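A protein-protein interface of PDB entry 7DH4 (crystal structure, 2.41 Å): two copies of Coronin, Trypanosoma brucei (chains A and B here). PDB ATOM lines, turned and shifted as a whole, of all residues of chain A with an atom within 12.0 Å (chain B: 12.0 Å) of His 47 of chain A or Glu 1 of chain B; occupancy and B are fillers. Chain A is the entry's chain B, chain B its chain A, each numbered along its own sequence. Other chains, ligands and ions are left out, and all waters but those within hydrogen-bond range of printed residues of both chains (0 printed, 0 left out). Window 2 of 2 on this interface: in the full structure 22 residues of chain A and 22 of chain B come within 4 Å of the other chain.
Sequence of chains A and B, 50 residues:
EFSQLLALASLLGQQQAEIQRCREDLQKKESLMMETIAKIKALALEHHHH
Of the 13 printed residues of chain A, 5 touch a printed residue of chain B. Hydrophobic or aromatic side chains of chain A that line the printed part of chain B: Ile 40, Leu 43 and His 47. Hydrophobic or aromatic side chains of chain B that line the printed part of chain A: Phe 2, Leu 5 and Leu 8. Among the printed residues, 10 pairs touch across the chains. Among the printed residues, no Asp or Glu carboxylate lies within 4 Å of a Lys or Arg side-chain nitrogen of the other chain.
Of the printed residues of chain B, His 47 of chain A touches Glu 1 (3.7 Å) and Phe 2 (3.1 Å). Of chain A, only His 47 comes within 4 Å of Glu 1 of chain B. Ala 44 of chain A touches just one residue of chain B: Leu 5 (3.9 Å). No residue of chain B comes within 4 Å of Glu 46 of chain A. No residue of chain B comes within 4 Å of His 48 of chain A. No residue of chain B comes within 4 Å of His 49 of chain A. No residue of chain B comes within 4 Å of His 50 of chain A. Of chain A, only His 47 comes within 4 Å of Phe 2 of chain B. No residue of chain A comes within 4 Å of Ser 3 of chain B. Of the printed residues of chain A, Ala 9 of chain B touches Ile 40 (3.9 Å). Of the printed residues of chain A, Leu 5 of chain B touches Ile 40 (3.7 Å), Leu 43 (3.5 Å) and Ala 44 (3.9 Å). Leu 6 of chain B touches none of the printed residues of chain A. Ala 38 of chain A touches none of the printed residues of chain B. The nearest residue of chain B that does not touch His 47 of chain A is Leu 5 of chain B (5.7 Å). The nearest printed residue of chain B that does not touch Lys 39 of chain A is Leu 5 of chain B (5.6 Å).
Leu 8 of chain B touches Lys 39 of chain A. Leu 5 of chain B touches Ile 40 of chain A (CD1 to O, 3.7 Å). CG1 of Ile 40 of chain A touches CB of Leu 8 of chain B (3.9 Å). Ile 40 of chain A touches Ala 9 of chain B (CD1 to N, 3.9 Å). Gln 4 of chain B touches Leu 43 of chain A. Leu 43 of chain A touches Leu 5 of chain B. Leu 8 of chain B touches Leu 43 of chain A (CD1 to CD2, 3.9 Å). Ala 44 of chain A touches Leu 5 of chain B. His 47 of chain A touches Glu 1 of chain B. CE1 of Phe 2 of chain B touches ND1 of His 47 of chain A, at 3.1 Å.
No position is printed for both chains. Of the 10 pairs that touch across the chains among the printed residues, none has its exchanged pair printed and touching as well.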
ATOM      1  N   ALA A  38      27.185 -14.480  16.187  1.00  0.00           N
ATOM      2  CA  ALA A  38      27.042 -15.451  17.267  1.00  0.00           C
ATOM      3  C   ALA A  38      26.317 -14.841  18.459  1.00  0.00           C
ATOM      4  O   ALA A  38      25.538 -15.522  19.137  1.00  0.00           O
ATOM      5  CB  ALA A  38      28.414 -15.980  17.685  1.00  0.00           C
ATOM      6  N   LYS A  39      26.561 -13.556  18.730  1.00  0.00           N
ATOM      7  CA  LYS A  39      25.821 -12.866  19.782  1.00  0.00           C
ATOM      8  C   LYS A  39      24.337 -12.791  19.448  1.00  0.00           C
ATOM      9  O   LYS A  39      23.487 -13.012  20.318  1.00  0.00           O
ATOM     10  CB  LYS A  39      26.387 -11.462  19.991  1.00  0.00           C
ATOM     11  CG  LYS A  39      27.580 -11.387  20.930  1.00  0.00           C
ATOM     12  CD  LYS A  39      27.935  -9.937  21.225  1.00  0.00           C
ATOM     13  CE  LYS A  39      28.936  -9.825  22.361  1.00  0.00           C
ATOM     14  NZ  LYS A  39      30.338  -9.960  21.880  1.00  0.00           N
ATOM     15  N   ILE A  40      24.009 -12.479  18.192  1.00  0.00           N
ATOM     16  CA  ILE A  40      22.608 -12.375  17.788  1.00  0.00           C
ATOM     17  C   ILE A  40      21.924 -13.731  17.888  1.00  0.00           C
ATOM     18  O   ILE A  40      20.806 -13.845  18.406  1.00  0.00           O
ATOM     19  CB  ILE A  40      22.502 -11.795  16.366  1.00  0.00           C
ATOM     20  CG1 ILE A  40      23.014 -10.354  16.330  1.00  0.00           C
ATOM     21  CG2 ILE A  40      21.067 -11.874  15.862  1.00  0.00           C
ATOM     22  CD1 ILE A  40      22.968  -9.726  14.953  1.00  0.00           C
ATOM     23  N   LYS A  41      22.586 -14.780  17.395  1.00  0.00           N
ATOM     24  CA  LYS A  41      22.006 -16.119  17.435  1.00  0.00           C
ATOM     25  C   LYS A  41      21.716 -16.550  18.867  1.00  0.00           C
ATOM     26  O   LYS A  41      20.605 -16.990  19.182  1.00  0.00           O
ATOM     27  CB  LYS A  41      22.941 -17.117  16.754  1.00  0.00           C
ATOM     28  CG  LYS A  41      22.308 -18.473  16.485  1.00  0.00           C
ATOM     29  CD  LYS A  41      23.351 -19.486  16.052  1.00  0.00           C
ATOM     30  CE  LYS A  41      23.598 -20.522  17.135  1.00  0.00           C
ATOM     31  NZ  LYS A  41      23.996 -21.834  16.552  1.00  0.00           N
ATOM     32  N   ALA A  42      22.712 -16.431  19.750  1.00  0.00           N
ATOM     33  CA  ALA A  42      22.516 -16.821  21.143  1.00  0.00           C
ATOM     34  C   ALA A  42      21.441 -15.978  21.814  1.00  0.00           C
ATOM     35  O   ALA A  42      20.740 -16.464  22.709  1.00  0.00           O
ATOM     36  CB  ALA A  42      23.833 -16.714  21.910  1.00  0.00           C
ATOM     37  N   LEU A  43      21.291 -14.719  21.397  1.00  0.00           N
ATOM     38  CA  LEU A  43      20.252 -13.871  21.971  1.00  0.00           C
ATOM     39  C   LEU A  43      18.870 -14.290  21.488  1.00  0.00           C
ATOM     40  O   LEU A  43      17.901 -14.253  22.256  1.00  0.00           O
ATOM     41  CB  LEU A  43      20.523 -12.407  21.629  1.00  0.00           C
ATOM     42  CG  LEU A  43      20.394 -11.410  22.780  1.00  0.00           C
ATOM     43  CD1 LEU A  43      21.041 -11.959  24.042  1.00  0.00           C
ATOM     44  CD2 LEU A  43      21.023 -10.086  22.391  1.00  0.00           C
ATOM     45  N   ALA A  44      18.755 -14.689  20.220  1.00  0.00           N
ATOM     46  CA  ALA A  44      17.486 -15.197  19.712  1.00  0.00           C
ATOM     47  C   ALA A  44      17.059 -16.450  20.470  1.00  0.00           C
ATOM     48  O   ALA A  44      15.883 -16.618  20.805  1.00  0.00           O
ATOM     49  CB  ALA A  44      17.593 -15.482  18.213  1.00  0.00           C
ATOM     50  N   LEU A  45      18.015 -17.340  20.751  1.00  0.00           N
ATOM     51  CA  LEU A  45      17.698 -18.574  21.461  1.00  0.00           C
ATOM     52  C   LEU A  45      17.241 -18.292  22.889  1.00  0.00           C
ATOM     53  O   LEU A  45      16.346 -18.971  23.404  1.00  0.00           O
ATOM     54  CB  LEU A  45      18.911 -19.503  21.462  1.00  0.00           C
ATOM     55  CG  LEU A  45      19.239 -20.206  20.142  1.00  0.00           C
ATOM     56  CD1 LEU A  45      20.468 -21.087  20.304  1.00  0.00           C
ATOM     57  CD2 LEU A  45      18.050 -21.020  19.663  1.00  0.00           C
ATOM     58  N   GLU A  46      17.853 -17.300  23.536  1.00  0.00           N
ATOM     59  CA  GLU A  46      17.468 -16.944  24.900  1.00  0.00           C
ATOM     60  C   GLU A  46      15.993 -16.572  24.977  1.00  0.00           C
ATOM     61  O   GLU A  46      15.266 -17.047  25.859  1.00  0.00           O
ATOM     62  CB  GLU A  46      18.334 -15.783  25.385  1.00  0.00           C
ATOM     63  CG  GLU A  46      19.453 -16.170  26.328  1.00  0.00           C
ATOM     64  CD  GLU A  46      20.453 -15.047  26.512  1.00  0.00           C
ATOM     65  OE1 GLU A  46      21.579 -15.155  25.981  1.00  0.00           O
ATOM     66  OE2 GLU A  46      20.105 -14.047  27.175  1.00  0.00           O
ATOM     67  N   HIS A  47      15.528 -15.725  24.058  1.00  0.00           N
ATOM     68  CA  HIS A  47      14.161 -15.214  24.127  1.00  0.00           C
ATOM     69  C   HIS A  47      13.138 -16.313  23.855  1.00  0.00           C
ATOM     70  O   HIS A  47      12.096 -16.376  24.525  1.00  0.00           O
ATOM     71  CB  HIS A  47      13.993 -14.047  23.141  1.00  0.00           C
ATOM     72  CG  HIS A  47      14.380 -12.708  23.702  1.00  0.00           C
ATOM     73  ND1 HIS A  47      14.439 -11.567  22.924  1.00  0.00           N
ATOM     74  CD2 HIS A  47      14.705 -12.326  24.955  1.00  0.00           C
ATOM     75  CE1 HIS A  47      14.800 -10.545  23.680  1.00  0.00           C
ATOM     76  NE2 HIS A  47      14.967 -10.974  24.915  1.00  0.00           N
ATOM     77  N   HIS A  48      13.409 -17.190  22.879  1.00  0.00           N
ATOM     78  CA  HIS A  48      12.485 -18.280  22.576  1.00  0.00           C
ATOM     79  C   HIS A  48      12.228 -19.154  23.802  1.00  0.00           C
ATOM     80  O   HIS A  48      11.114 -19.657  23.995  1.00  0.00           O
ATOM     81  CB  HIS A  48      13.024 -19.118  21.415  1.00  0.00           C
ATOM     82  CG  HIS A  48      12.445 -20.497  21.343  1.00  0.00           C
ATOM     83  ND1 HIS A  48      13.163 -21.625  21.684  1.00  0.00           N
ATOM     84  CD2 HIS A  48      11.213 -20.930  20.993  1.00  0.00           C
ATOM     85  CE1 HIS A  48      12.401 -22.692  21.531  1.00  0.00           C
ATOM     86  NE2 HIS A  48      11.211 -22.299  21.115  1.00  0.00           N
ATOM     87  N   HIS A  49      13.248 -19.338  24.646  1.00  0.00           N
ATOM     88  CA  HIS A  49      13.101 -20.042  25.915  1.00  0.00           C
ATOM     89  C   HIS A  49      12.514 -19.161  27.014  1.00  0.00           C
ATOM     90  O   HIS A  49      12.616 -19.520  28.195  1.00  0.00           O
ATOM     91  CB  HIS A  49      14.451 -20.609  26.357  1.00  0.00           C
ATOM     92  CG  HIS A  49      15.010 -21.630  25.416  1.00  0.00           C
ATOM     93  ND1 HIS A  49      14.281 -22.150  24.371  1.00  0.00           N
ATOM     94  CD2 HIS A  49      16.225 -22.227  25.365  1.00  0.00           C
ATOM     95  CE1 HIS A  49      15.023 -23.026  23.713  1.00  0.00           C
ATOM     96  NE2 HIS A  49      16.205 -23.091  24.297  1.00  0.00           N
ATOM     97  N   HIS A  50      11.922 -18.025  26.648  1.00  0.00           N
ATOM     98  CA  HIS A  50      11.236 -17.136  27.586  1.00  0.00           C
ATOM     99  C   HIS A  50      12.150 -16.685  28.722  1.00  0.00           C
ATOM    100  O   HIS A  50      12.668 -15.566  28.707  1.00  0.00           O
ATOM    101  CB  HIS A  50       9.988 -17.824  28.148  1.00  0.00           C
ATOM    102  CG  HIS A  50       9.057 -18.340  27.093  1.00  0.00           C
ATOM    103  ND1 HIS A  50       8.843 -17.680  25.903  1.00  0.00           N
ATOM    104  CD2 HIS A  50       8.290 -19.455  27.047  1.00  0.00           C
ATOM    105  CE1 HIS A  50       7.982 -18.363  25.169  1.00  0.00           C
ATOM    106  NE2 HIS A  50       7.631 -19.445  25.841  1.00  0.00           N
ATOM    107  N   GLU B   1      14.232  -4.926  26.669  1.00  0.00           N
ATOM    108  CA  GLU B   1      13.901  -6.289  26.262  1.00  0.00           C
ATOM    109  C   GLU B   1      14.720  -6.707  25.043  1.00  0.00           C
ATOM    110  O   GLU B   1      15.808  -7.273  25.175  1.00  0.00           O
ATOM    111  CB  GLU B   1      12.413  -6.407  25.971  1.00  0.00           C
ATOM    112  N   PHE B   2      14.180  -6.427  23.859  1.00  0.00           N
ATOM    113  CA  PHE B   2      14.839  -6.668  22.578  1.00  0.00           C
ATOM    114  C   PHE B   2      15.907  -5.625  22.255  1.00  0.00           C
ATOM    115  O   PHE B   2      16.380  -5.587  21.113  1.00  0.00           O
ATOM    116  CB  PHE B   2      13.788  -6.688  21.461  1.00  0.00           C
ATOM    117  CG  PHE B   2      13.419  -8.056  20.971  1.00  0.00           C
ATOM    118  CD1 PHE B   2      14.396  -8.955  20.592  1.00  0.00           C
ATOM    119  CD2 PHE B   2      12.091  -8.456  20.925  1.00  0.00           C
ATOM    120  CE1 PHE B   2      14.057 -10.211  20.128  1.00  0.00           C
ATOM    121  CE2 PHE B   2      11.749  -9.708  20.478  1.00  0.00           C
ATOM    122  CZ  PHE B   2      12.726 -10.593  20.080  1.00  0.00           C
ATOM    123  N   SER B   3      16.281  -4.774  23.216  1.00  0.00           N
ATOM    124  CA  SER B   3      17.243  -3.711  22.940  1.00  0.00           C
ATOM    125  C   SER B   3      18.626  -4.277  22.647  1.00  0.00           C
ATOM    126  O   SER B   3      19.324  -3.794  21.749  1.00  0.00           O
ATOM    127  CB  SER B   3      17.306  -2.742  24.121  1.00  0.00           C
ATOM    128  OG  SER B   3      17.202  -3.434  25.353  1.00  0.00           O
ATOM    129  N   GLN B   4      19.044  -5.285  23.415  1.00  0.00           N
ATOM    130  CA  GLN B   4      20.358  -5.892  23.223  1.00  0.00           C
ATOM    131  C   GLN B   4      20.529  -6.397  21.797  1.00  0.00           C
ATOM    132  O   GLN B   4      21.559  -6.154  21.156  1.00  0.00           O
ATOM    133  CB  GLN B   4      20.541  -7.032  24.226  1.00  0.00           C
ATOM    134  CG  GLN B   4      21.966  -7.292  24.666  1.00  0.00           C
ATOM    135  CD  GLN B   4      22.022  -8.059  25.973  1.00  0.00           C
ATOM    136  OE1 GLN B   4      20.988  -8.396  26.550  1.00  0.00           O
ATOM    137  NE2 GLN B   4      23.230  -8.346  26.444  1.00  0.00           N
ATOM    138  N   LEU B   5      19.517  -7.094  21.274  1.00  0.00           N
ATOM    139  CA  LEU B   5      19.618  -7.681  19.944  1.00  0.00           C
ATOM    140  C   LEU B   5      19.616  -6.609  18.860  1.00  0.00           C
ATOM    141  O   LEU B   5      20.433  -6.650  17.932  1.00  0.00           O
ATOM    142  CB  LEU B   5      18.474  -8.673  19.723  1.00  0.00           C
ATOM    143  CG  LEU B   5      18.562  -9.575  18.493  1.00  0.00           C
ATOM    144  CD1 LEU B   5      18.488 -11.041  18.892  1.00  0.00           C
ATOM    145  CD2 LEU B   5      17.460  -9.234  17.505  1.00  0.00           C
ATOM    146  N   LEU B   6      18.704  -5.638  18.965  1.00  0.00           N
ATOM    147  CA  LEU B   6      18.601  -4.599  17.944  1.00  0.00           C
ATOM    148  C   LEU B   6      19.905  -3.828  17.802  1.00  0.00           C
ATOM    149  O   LEU B   6      20.322  -3.496  16.684  1.00  0.00           O
ATOM    150  CB  LEU B   6      17.453  -3.650  18.282  1.00  0.00           C
ATOM    151  CG  LEU B   6      16.049  -4.228  18.119  1.00  0.00           C
ATOM    152  CD1 LEU B   6      15.030  -3.377  18.859  1.00  0.00           C
ATOM    153  CD2 LEU B   6      15.692  -4.344  16.647  1.00  0.00           C
ATOM    154  N   ALA B   7      20.567  -3.533  18.924  1.00  0.00           N
ATOM    155  CA  ALA B   7      21.833  -2.812  18.870  1.00  0.00           C
ATOM    156  C   ALA B   7      22.904  -3.627  18.153  1.00  0.00           C
ATOM    157  O   ALA B   7      23.742  -3.069  17.435  1.00  0.00           O
ATOM    158  CB  ALA B   7      22.289  -2.448  20.282  1.00  0.00           C
ATOM    159  N   LEU B   8      22.893  -4.950  18.336  1.00  0.00           N
ATOM    160  CA  LEU B   8      23.883  -5.789  17.672  1.00  0.00           C
ATOM    161  C   LEU B   8      23.587  -5.941  16.186  1.00  0.00           C
ATOM    162  O   LEU B   8      24.517  -6.024  15.377  1.00  0.00           O
ATOM    163  CB  LEU B   8      23.954  -7.159  18.344  1.00  0.00           C
ATOM    164  CG  LEU B   8      24.541  -7.161  19.759  1.00  0.00           C
ATOM    165  CD1 LEU B   8      23.981  -8.305  20.599  1.00  0.00           C
ATOM    166  CD2 LEU B   8      26.057  -7.213  19.699  1.00  0.00           C
ATOM    167  N   ALA B   9      22.309  -5.987  15.809  1.00  0.00           N
ATOM    168  CA  ALA B   9      21.962  -5.994  14.393  1.00  0.00           C
ATOM    169  C   ALA B   9      22.351  -4.680  13.731  1.00  0.00           C
ATOM    170  O   ALA B   9      22.801  -4.666  12.580  1.00  0.00           O
ATOM    171  CB  ALA B   9      20.468  -6.265  14.218  1.00  0.00           C
